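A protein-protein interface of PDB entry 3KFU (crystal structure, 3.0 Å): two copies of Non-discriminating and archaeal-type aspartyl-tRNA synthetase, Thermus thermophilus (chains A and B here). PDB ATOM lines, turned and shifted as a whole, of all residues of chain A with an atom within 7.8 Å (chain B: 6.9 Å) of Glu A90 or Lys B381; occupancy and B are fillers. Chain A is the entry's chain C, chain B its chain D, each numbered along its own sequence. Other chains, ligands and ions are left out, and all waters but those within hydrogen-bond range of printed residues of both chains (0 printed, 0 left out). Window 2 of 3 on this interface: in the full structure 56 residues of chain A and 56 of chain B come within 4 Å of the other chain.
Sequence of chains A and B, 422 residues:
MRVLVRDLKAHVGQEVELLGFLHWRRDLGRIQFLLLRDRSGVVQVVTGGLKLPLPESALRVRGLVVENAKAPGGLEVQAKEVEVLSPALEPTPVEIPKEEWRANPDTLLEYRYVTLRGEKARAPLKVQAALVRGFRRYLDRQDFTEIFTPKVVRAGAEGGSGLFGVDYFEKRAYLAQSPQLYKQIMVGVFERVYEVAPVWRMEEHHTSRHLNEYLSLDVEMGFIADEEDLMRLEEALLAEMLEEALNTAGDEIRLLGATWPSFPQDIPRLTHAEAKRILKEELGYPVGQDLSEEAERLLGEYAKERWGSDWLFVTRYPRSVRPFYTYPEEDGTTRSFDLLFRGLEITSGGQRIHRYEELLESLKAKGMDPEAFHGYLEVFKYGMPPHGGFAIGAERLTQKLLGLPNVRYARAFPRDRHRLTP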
ATOM      1  N   LEU A  54      -1.253  35.063   0.389  1.00  0.00           N
ATOM      2  CA  LEU A  54      -0.798  35.432   1.717  1.00  0.00           C
ATOM      3  C   LEU A  54       0.474  36.262   1.582  1.00  0.00           C
ATOM      4  O   LEU A  54       1.162  36.189   0.563  1.00  0.00           O
ATOM      5  CB  LEU A  54      -0.534  34.182   2.556  1.00  0.00           C
ATOM      6  CG  LEU A  54      -1.766  33.348   2.908  1.00  0.00           C
ATOM      7  CD1 LEU A  54      -1.370  32.019   3.533  1.00  0.00           C
ATOM      8  CD2 LEU A  54      -2.683  34.126   3.837  1.00  0.00           C
ATOM      9  N   PRO A  55       0.782  37.071   2.601  1.00  0.00           N
ATOM     10  CA  PRO A  55       2.024  37.845   2.572  1.00  0.00           C
ATOM     11  C   PRO A  55       3.228  36.936   2.338  1.00  0.00           C
ATOM     12  O   PRO A  55       3.172  35.748   2.655  1.00  0.00           O
ATOM     13  CB  PRO A  55       2.081  38.456   3.973  1.00  0.00           C
ATOM     14  CG  PRO A  55       0.655  38.556   4.389  1.00  0.00           C
ATOM     15  CD  PRO A  55      -0.023  37.354   3.802  1.00  0.00           C
ATOM     16  N   GLU A  56       4.293  37.499   1.779  1.00  0.00           N
ATOM     17  CA  GLU A  56       5.522  36.759   1.502  1.00  0.00           C
ATOM     18  C   GLU A  56       5.414  35.879   0.258  1.00  0.00           C
ATOM     19  O   GLU A  56       6.105  34.869   0.143  1.00  0.00           O
ATOM     20  CB  GLU A  56       5.952  35.932   2.719  1.00  0.00           C
ATOM     21  CG  GLU A  56       7.265  36.386   3.324  1.00  0.00           C
ATOM     22  CD  GLU A  56       7.332  37.891   3.496  1.00  0.00           C
ATOM     23  OE1 GLU A  56       6.410  38.466   4.113  1.00  0.00           O
ATOM     24  OE2 GLU A  56       8.306  38.499   3.005  1.00  0.00           O
ATOM     25  N   SER A  57       4.547  36.270  -0.671  1.00  0.00           N
ATOM     26  CA  SER A  57       4.415  35.564  -1.940  1.00  0.00           C
ATOM     27  C   SER A  57       5.193  36.282  -3.035  1.00  0.00           C
ATOM     28  O   SER A  57       5.132  37.507  -3.147  1.00  0.00           O
ATOM     29  CB  SER A  57       2.945  35.448  -2.345  1.00  0.00           C
ATOM     30  OG  SER A  57       2.231  34.612  -1.452  1.00  0.00           O
ATOM     31  N   SER A  86       4.996  32.731  -6.992  1.00  0.00           N
ATOM     32  CA  SER A  86       5.073  31.703  -5.961  1.00  0.00           C
ATOM     33  C   SER A  86       4.224  32.081  -4.753  1.00  0.00           C
ATOM     34  O   SER A  86       4.572  32.993  -4.004  1.00  0.00           O
ATOM     35  CB  SER A  86       6.526  31.484  -5.533  1.00  0.00           C
ATOM     36  OG  SER A  86       6.625  30.438  -4.585  1.00  0.00           O
ATOM     37  N   PRO A  87       3.098  31.376  -4.566  1.00  0.00           N
ATOM     38  CA  PRO A  87       2.146  31.640  -3.482  1.00  0.00           C
ATOM     39  C   PRO A  87       2.628  31.088  -2.149  1.00  0.00           C
ATOM     40  O   PRO A  87       3.213  30.005  -2.105  1.00  0.00           O
ATOM     41  CB  PRO A  87       0.889  30.872  -3.920  1.00  0.00           C
ATOM     42  CG  PRO A  87       1.146  30.433  -5.338  1.00  0.00           C
ATOM     43  CD  PRO A  87       2.623  30.307  -5.455  1.00  0.00           C
ATOM     44  N   ALA A  88       2.380  31.828  -1.074  1.00  0.00           N
ATOM     45  CA  ALA A  88       2.682  31.344   0.265  1.00  0.00           C
ATOM     46  C   ALA A  88       1.554  30.428   0.735  1.00  0.00           C
ATOM     47  O   ALA A  88       0.376  30.759   0.601  1.00  0.00           O
ATOM     48  CB  ALA A  88       2.874  32.509   1.228  1.00  0.00           C
ATOM     49  N   LEU A  89       1.922  29.271   1.273  1.00  0.00           N
ATOM     50  CA  LEU A  89       0.940  28.282   1.699  1.00  0.00           C
ATOM     51  C   LEU A  89       0.261  28.679   3.003  1.00  0.00           C
ATOM     52  O   LEU A  89      -0.957  28.572   3.138  1.00  0.00           O
ATOM     53  CB  LEU A  89       1.596  26.909   1.856  1.00  0.00           C
ATOM     54  CG  LEU A  89       2.369  26.389   0.646  1.00  0.00           C
ATOM     55  CD1 LEU A  89       2.646  24.902   0.801  1.00  0.00           C
ATOM     56  CD2 LEU A  89       1.597  26.664  -0.637  1.00  0.00           C
ATOM     57  N   GLU A  90       1.056  29.134   3.963  1.00  0.00           N
ATOM     58  CA  GLU A  90       0.541  29.474   5.281  1.00  0.00           C
ATOM     59  C   GLU A  90       0.949  30.887   5.667  1.00  0.00           C
ATOM     60  O   GLU A  90       1.789  31.498   5.009  1.00  0.00           O
ATOM     61  CB  GLU A  90       1.061  28.482   6.325  1.00  0.00           C
ATOM     62  CG  GLU A  90       0.711  27.030   6.042  1.00  0.00           C
ATOM     63  CD  GLU A  90       1.280  26.082   7.081  1.00  0.00           C
ATOM     64  OE1 GLU A  90       1.750  26.563   8.134  1.00  0.00           O
ATOM     65  OE2 GLU A  90       1.259  24.854   6.846  1.00  0.00           O
ATOM     66  N   PRO A  91       0.341  31.420   6.735  1.00  0.00           N
ATOM     67  CA  PRO A  91       0.754  32.715   7.286  1.00  0.00           C
ATOM     68  C   PRO A  91       2.093  32.586   8.000  1.00  0.00           C
ATOM     69  O   PRO A  91       2.339  31.573   8.654  1.00  0.00           O
ATOM     70  CB  PRO A  91      -0.348  33.032   8.304  1.00  0.00           C
ATOM     71  CG  PRO A  91      -1.489  32.130   7.951  1.00  0.00           C
ATOM     72  CD  PRO A  91      -0.862  30.896   7.400  1.00  0.00           C
ATOM     73  N   THR A  92       2.948  33.596   7.872  1.00  0.00           N
ATOM     74  CA  THR A  92       4.248  33.578   8.531  1.00  0.00           C
ATOM     75  C   THR A  92       4.086  33.490  10.042  1.00  0.00           C
ATOM     76  O   THR A  92       3.125  34.021  10.595  1.00  0.00           O
ATOM     77  CB  THR A  92       5.078  34.827   8.181  1.00  0.00           C
ATOM     78  OG1 THR A  92       4.282  36.003   8.370  1.00  0.00           O
ATOM     79  CG2 THR A  92       5.542  34.767   6.737  1.00  0.00           C
ATOM     80  N   PRO A  93       5.030  32.809  10.714  1.00  0.00           N
ATOM     81  CA  PRO A  93       5.009  32.642  12.172  1.00  0.00           C
ATOM     82  C   PRO A  93       5.000  33.992  12.875  1.00  0.00           C
ATOM     83  O   PRO A  93       4.407  34.139  13.942  1.00  0.00           O
ATOM     84  CB  PRO A  93       6.326  31.916  12.458  1.00  0.00           C
ATOM     85  CG  PRO A  93       6.659  31.219  11.186  1.00  0.00           C
ATOM     86  CD  PRO A  93       6.184  32.132  10.098  1.00  0.00           C
ATOM     87  N   TYR A 113      14.834  32.004   9.431  1.00  0.00           N
ATOM     88  CA  TYR A 113      14.742  31.674   8.009  1.00  0.00           C
ATOM     89  C   TYR A 113      13.685  32.472   7.253  1.00  0.00           C
ATOM     90  O   TYR A 113      13.488  32.273   6.054  1.00  0.00           O
ATOM     91  CB  TYR A 113      14.494  30.176   7.816  1.00  0.00           C
ATOM     92  CG  TYR A 113      13.179  29.686   8.380  1.00  0.00           C
ATOM     93  CD1 TYR A 113      12.006  29.784   7.644  1.00  0.00           C
ATOM     94  CD2 TYR A 113      13.114  29.112   9.644  1.00  0.00           C
ATOM     95  CE1 TYR A 113      10.802  29.331   8.153  1.00  0.00           C
ATOM     96  CE2 TYR A 113      11.915  28.657  10.161  1.00  0.00           C
ATOM     97  CZ  TYR A 113      10.762  28.769   9.413  1.00  0.00           C
ATOM     98  OH  TYR A 113       9.566  28.317   9.926  1.00  0.00           O
ATOM     99  N   ARG A 117      14.055  38.360   6.429  1.00  0.00           N
ATOM    100  CA  ARG A 117      13.599  39.060   5.233  1.00  0.00           C
ATOM    101  C   ARG A 117      13.236  40.516   5.508  1.00  0.00           C
ATOM    102  O   ARG A 117      13.313  41.358   4.613  1.00  0.00           O
ATOM    103  CB  ARG A 117      12.410  38.332   4.606  1.00  0.00           C
ATOM    104  CG  ARG A 117      12.748  36.949   4.081  1.00  0.00           C
ATOM    105  CD  ARG A 117      11.551  36.288   3.425  1.00  0.00           C
ATOM    106  NE  ARG A 117      11.856  34.924   3.008  1.00  0.00           N
ATOM    107  CZ  ARG A 117      11.012  34.139   2.349  1.00  0.00           C
ATOM    108  NH1 ARG A 117       9.807  34.584   2.025  1.00  0.00           N
ATOM    109  NH2 ARG A 117      11.374  32.909   2.011  1.00  0.00           N
ATOM    110  N   HIS B 354      11.188  25.157  -5.898  1.00  0.00           N
ATOM    111  CA  HIS B 354      10.774  26.238  -5.009  1.00  0.00           C
ATOM    112  C   HIS B 354       9.373  26.017  -4.450  1.00  0.00           C
ATOM    113  O   HIS B 354       8.898  26.792  -3.620  1.00  0.00           O
ATOM    114  CB  HIS B 354      10.851  27.585  -5.729  1.00  0.00           C
ATOM    115  CG  HIS B 354      10.010  27.657  -6.964  1.00  0.00           C
ATOM    116  ND1 HIS B 354       8.729  28.166  -6.966  1.00  0.00           N
ATOM    117  CD2 HIS B 354      10.266  27.281  -8.241  1.00  0.00           C
ATOM    118  CE1 HIS B 354       8.234  28.102  -8.188  1.00  0.00           C
ATOM    119  NE2 HIS B 354       9.146  27.569  -8.980  1.00  0.00           N
ATOM    120  N   ARG B 355       8.716  24.959  -4.909  1.00  0.00           N
ATOM    121  CA  ARG B 355       7.393  24.608  -4.406  1.00  0.00           C
ATOM    122  C   ARG B 355       7.523  23.600  -3.268  1.00  0.00           C
ATOM    123  O   ARG B 355       8.105  22.529  -3.444  1.00  0.00           O
ATOM    124  CB  ARG B 355       6.527  24.033  -5.528  1.00  0.00           C
ATOM    125  CG  ARG B 355       6.507  24.877  -6.796  1.00  0.00           C
ATOM    126  CD  ARG B 355       5.817  26.218  -6.583  1.00  0.00           C
ATOM    127  NE  ARG B 355       4.371  26.081  -6.427  1.00  0.00           N
ATOM    128  CZ  ARG B 355       3.736  26.104  -5.260  1.00  0.00           C
ATOM    129  NH1 ARG B 355       4.416  26.264  -4.133  1.00  0.00           N
ATOM    130  NH2 ARG B 355       2.417  25.970  -5.219  1.00  0.00           N
ATOM    131  N   TYR B 356       6.987  23.952  -2.104  1.00  0.00           N
ATOM    132  CA  TYR B 356       7.085  23.098  -0.923  1.00  0.00           C
ATOM    133  C   TYR B 356       6.673  21.657  -1.203  1.00  0.00           C
ATOM    134  O   TYR B 356       7.387  20.718  -0.854  1.00  0.00           O
ATOM    135  CB  TYR B 356       6.242  23.666   0.221  1.00  0.00           C
ATOM    136  CG  TYR B 356       6.105  22.729   1.399  1.00  0.00           C
ATOM    137  CD1 TYR B 356       7.098  22.652   2.369  1.00  0.00           C
ATOM    138  CD2 TYR B 356       4.984  21.925   1.545  1.00  0.00           C
ATOM    139  CE1 TYR B 356       6.977  21.796   3.451  1.00  0.00           C
ATOM    140  CE2 TYR B 356       4.854  21.067   2.622  1.00  0.00           C
ATOM    141  CZ  TYR B 356       5.853  21.007   3.572  1.00  0.00           C
ATOM    142  OH  TYR B 356       5.728  20.155   4.646  1.00  0.00           O
ATOM    143  N   HIS B 374      12.540  18.363   8.005  1.00  0.00           N
ATOM    144  CA  HIS B 374      11.476  19.265   8.439  1.00  0.00           C
ATOM    145  C   HIS B 374      11.957  20.702   8.650  1.00  0.00           C
ATOM    146  O   HIS B 374      11.194  21.649   8.464  1.00  0.00           O
ATOM    147  CB  HIS B 374      10.814  18.739   9.713  1.00  0.00           C
ATOM    148  CG  HIS B 374       9.596  19.509  10.123  1.00  0.00           C
ATOM    149  ND1 HIS B 374       9.657  20.624  10.928  1.00  0.00           N
ATOM    150  CD2 HIS B 374       8.287  19.323   9.833  1.00  0.00           C
ATOM    151  CE1 HIS B 374       8.437  21.093  11.120  1.00  0.00           C
ATOM    152  NE2 HIS B 374       7.587  20.322  10.467  1.00  0.00           N
ATOM    153  N   LEU B 377      12.637  22.349   4.836  1.00  0.00           N
ATOM    154  CA  LEU B 377      11.450  22.661   4.047  1.00  0.00           C
ATOM    155  C   LEU B 377      10.702  23.895   4.538  1.00  0.00           C
ATOM    156  O   LEU B 377      10.035  24.573   3.756  1.00  0.00           O
ATOM    157  CB  LEU B 377      10.496  21.468   4.056  1.00  0.00           C
ATOM    158  CG  LEU B 377      11.117  20.110   3.730  1.00  0.00           C
ATOM    159  CD1 LEU B 377      10.102  18.995   3.925  1.00  0.00           C
ATOM    160  CD2 LEU B 377      11.664  20.107   2.316  1.00  0.00           C
ATOM    161  N   GLU B 378      10.802  24.172   5.834  1.00  0.00           N
ATOM    162  CA  GLU B 378      10.019  25.239   6.455  1.00  0.00           C
ATOM    163  C   GLU B 378       9.980  26.531   5.641  1.00  0.00           C
ATOM    164  O   GLU B 378       8.937  27.172   5.535  1.00  0.00           O
ATOM    165  CB  GLU B 378      10.515  25.515   7.878  1.00  0.00           C
ATOM    166  CG  GLU B 378       9.963  24.552   8.917  1.00  0.00           C
ATOM    167  CD  GLU B 378       8.454  24.653   9.055  1.00  0.00           C
ATOM    168  OE1 GLU B 378       7.745  23.751   8.559  1.00  0.00           O
ATOM    169  OE2 GLU B 378       7.977  25.636   9.659  1.00  0.00           O
ATOM    170  N   VAL B 379      11.114  26.904   5.059  1.00  0.00           N
ATOM    171  CA  VAL B 379      11.198  28.154   4.315  1.00  0.00           C
ATOM    172  C   VAL B 379      10.378  28.109   3.023  1.00  0.00           C
ATOM    173  O   VAL B 379       9.891  29.136   2.548  1.00  0.00           O
ATOM    174  CB  VAL B 379      12.663  28.523   3.989  1.00  0.00           C
ATOM    175  CG1 VAL B 379      13.175  27.690   2.829  1.00  0.00           C
ATOM    176  CG2 VAL B 379      12.778  30.000   3.667  1.00  0.00           C
ATOM    177  N   PHE B 380      10.217  26.917   2.460  1.00  0.00           N
ATOM    178  CA  PHE B 380       9.523  26.769   1.185  1.00  0.00           C
ATOM    179  C   PHE B 380       8.008  26.835   1.330  1.00  0.00           C
ATOM    180  O   PHE B 380       7.278  26.784   0.340  1.00  0.00           O
ATOM    181  CB  PHE B 380       9.949  25.478   0.483  1.00  0.00           C
ATOM    182  CG  PHE B 380      11.379  25.486   0.031  1.00  0.00           C
ATOM    183  CD1 PHE B 380      12.396  25.112   0.895  1.00  0.00           C
ATOM    184  CD2 PHE B 380      11.708  25.878  -1.254  1.00  0.00           C
ATOM    185  CE1 PHE B 380      13.715  25.125   0.481  1.00  0.00           C
ATOM    186  CE2 PHE B 380      13.025  25.893  -1.674  1.00  0.00           C
ATOM    187  CZ  PHE B 380      14.030  25.515  -0.807  1.00  0.00           C
ATOM    188  N   LYS B 381       7.538  26.948   2.567  1.00  0.00           N
ATOM    189  CA  LYS B 381       6.119  27.155   2.820  1.00  0.00           C
ATOM    190  C   LYS B 381       5.742  28.598   2.511  1.00  0.00           C
ATOM    191  O   LYS B 381       4.577  28.911   2.277  1.00  0.00           O
ATOM    192  CB  LYS B 381       5.774  26.842   4.279  1.00  0.00           C
ATOM    193  CG  LYS B 381       5.775  25.366   4.641  1.00  0.00           C
ATOM    194  CD  LYS B 381       5.279  25.166   6.066  1.00  0.00           C
ATOM    195  CE  LYS B 381       5.197  23.697   6.434  1.00  0.00           C
ATOM    196  NZ  LYS B 381       4.691  23.508   7.822  1.00  0.00           N
ATOM    197  N   TYR B 382       6.739  29.477   2.510  1.00  0.00           N
ATOM    198  CA  TYR B 382       6.489  30.908   2.394  1.00  0.00           C
ATOM    199  C   TYR B 382       7.053  31.516   1.111  1.00  0.00           C
ATOM    200  O   TYR B 382       8.118  32.137   1.122  1.00  0.00           O
ATOM    201  CB  TYR B 382       7.054  31.641   3.612  1.00  0.00           C
ATOM    202  CG  TYR B 382       6.705  30.983   4.925  1.00  0.00           C
ATOM    203  CD1 TYR B 382       5.496  31.242   5.557  1.00  0.00           C
ATOM    204  CD2 TYR B 382       7.585  30.097   5.535  1.00  0.00           C
ATOM    205  CE1 TYR B 382       5.175  30.639   6.760  1.00  0.00           C
ATOM    206  CE2 TYR B 382       7.272  29.491   6.737  1.00  0.00           C
ATOM    207  CZ  TYR B 382       6.067  29.764   7.344  1.00  0.00           C
ATOM    208  OH  TYR B 382       5.758  29.161   8.540  1.00  0.00           O
ATOM    209  N   GLY B 383       6.326  31.332   0.013  1.00  0.00           N
ATOM    210  CA  GLY B 383       6.630  31.978  -1.252  1.00  0.00           C
ATOM    211  C   GLY B 383       8.094  32.035  -1.640  1.00  0.00           C
ATOM    212  O   GLY B 383       8.736  33.080  -1.537  1.00  0.00           O
ATOM    213  N   MET B 384       8.623  30.909  -2.098  1.00  0.00           N
ATOM    214  CA  MET B 384      10.005  30.857  -2.542  1.00  0.00           C
ATOM    215  C   MET B 384      10.069  31.152  -4.033  1.00  0.00           C
ATOM    216  O   MET B 384       9.395  30.497  -4.827  1.00  0.00           O
ATOM    217  CB  MET B 384      10.611  29.487  -2.245  1.00  0.00           C
ATOM    218  CG  MET B 384      12.123  29.488  -2.208  1.00  0.00           C
ATOM    219  SD  MET B 384      12.757  30.543  -0.895  1.00  0.00           S
ATOM    220  CE  MET B 384      14.507  30.505  -1.262  1.00  0.00           C
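Gly B383 touches Glu A56 (CA to O, 3.3 Å). O of Ser A86 touches CA of Gly B383, 3.6 Å away. Ala A88 touches Lys B381. O of Glu A90 touches CD1 of Tyr B382, 3.8 Å away. Thr A92 touches Tyr B382 (CA to CE1, 3.6 Å). Pro A93 touches Tyr B382. CG2 of Val B379 touches O of Tyr A113, 3.4 Å away. Tyr A113 touches Tyr B382. Arg A117 touches Val B379 (NH2 to CG2, 3.6 Å). Met B384 touches Arg A117 (SD to NH2, 3.99 Å).
No position is printed for both chains. Of the 21 pairs that touch across the chains among the printed residues, none has its exchanged pair printed and touching as well.
A ring nitrogen (ND1) of His B354 lies within hydrogen-bond range of the backbone carbonyl oxygen (O) of Met B384 (3.2 Å). N of Ala A88 sits at hydrogen-bond distance from OG of Ser A57 (2.8 Å). OE1 of Glu B378 lies within salt-bridge range of NZ of Lys B381.
Ser A57 touches none of the printed residues of chain B. Glu A90 touches just these residues of chain B: Lys B381 (3.8 Å) and Tyr B382 (3.8 Å). Printed residues of chain B within 4 Å of Pro A91: Tyr B382. Printed residues of chain B within 4 Å of Tyr A113: Glu B378, Val B379 and Tyr B382. His B374 touches none of the printed residues of chain A. Of the printed residues of chain A, Glu B378 touches Tyr A113. Of the printed residues of chain A, Val B379 touches Tyr A113 and Arg A117. Lys B381 touches just these residues of chain A: Ala A88, Leu A89 and Glu A90. Of the printed residues of chain A, Met B384 touches Ser A86 (2.8 Å) and Arg A117 (3.99 Å). The nearest residue of chain A that does not touch Lys B381 is Pro A87 (4.7 Å).
The side-chain carboxylate (OE2) of Glu A90 lies within salt-bridge range of the side-chain amino group (NZ) of Lys B381. The side-chain hydroxyl of Tyr A113 sits at hydrogen-bond distance from the side-chain carboxylate of Glu B378 (3.1 Å). OG of Ser A86 lies within hydrogen-bond range of O of Met B384, at 2.8 Å. O of Tyr B382 lies within hydrogen-bond range of NH1 of Arg A117 (3.1 Å). N of Leu A89 lies within hydrogen-bond range of O of Lys B381.
Of the 14 printed residues of chain A, 11 touch a printed residue of chain B. Printed residues of chain A that touch a printed residue of chain B: Glu A56, Ser A86, Pro A87, Ala A88, Leu A89, Glu A90, Pro A91, Thr A92, Pro A93, Tyr A113 and Arg A117.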
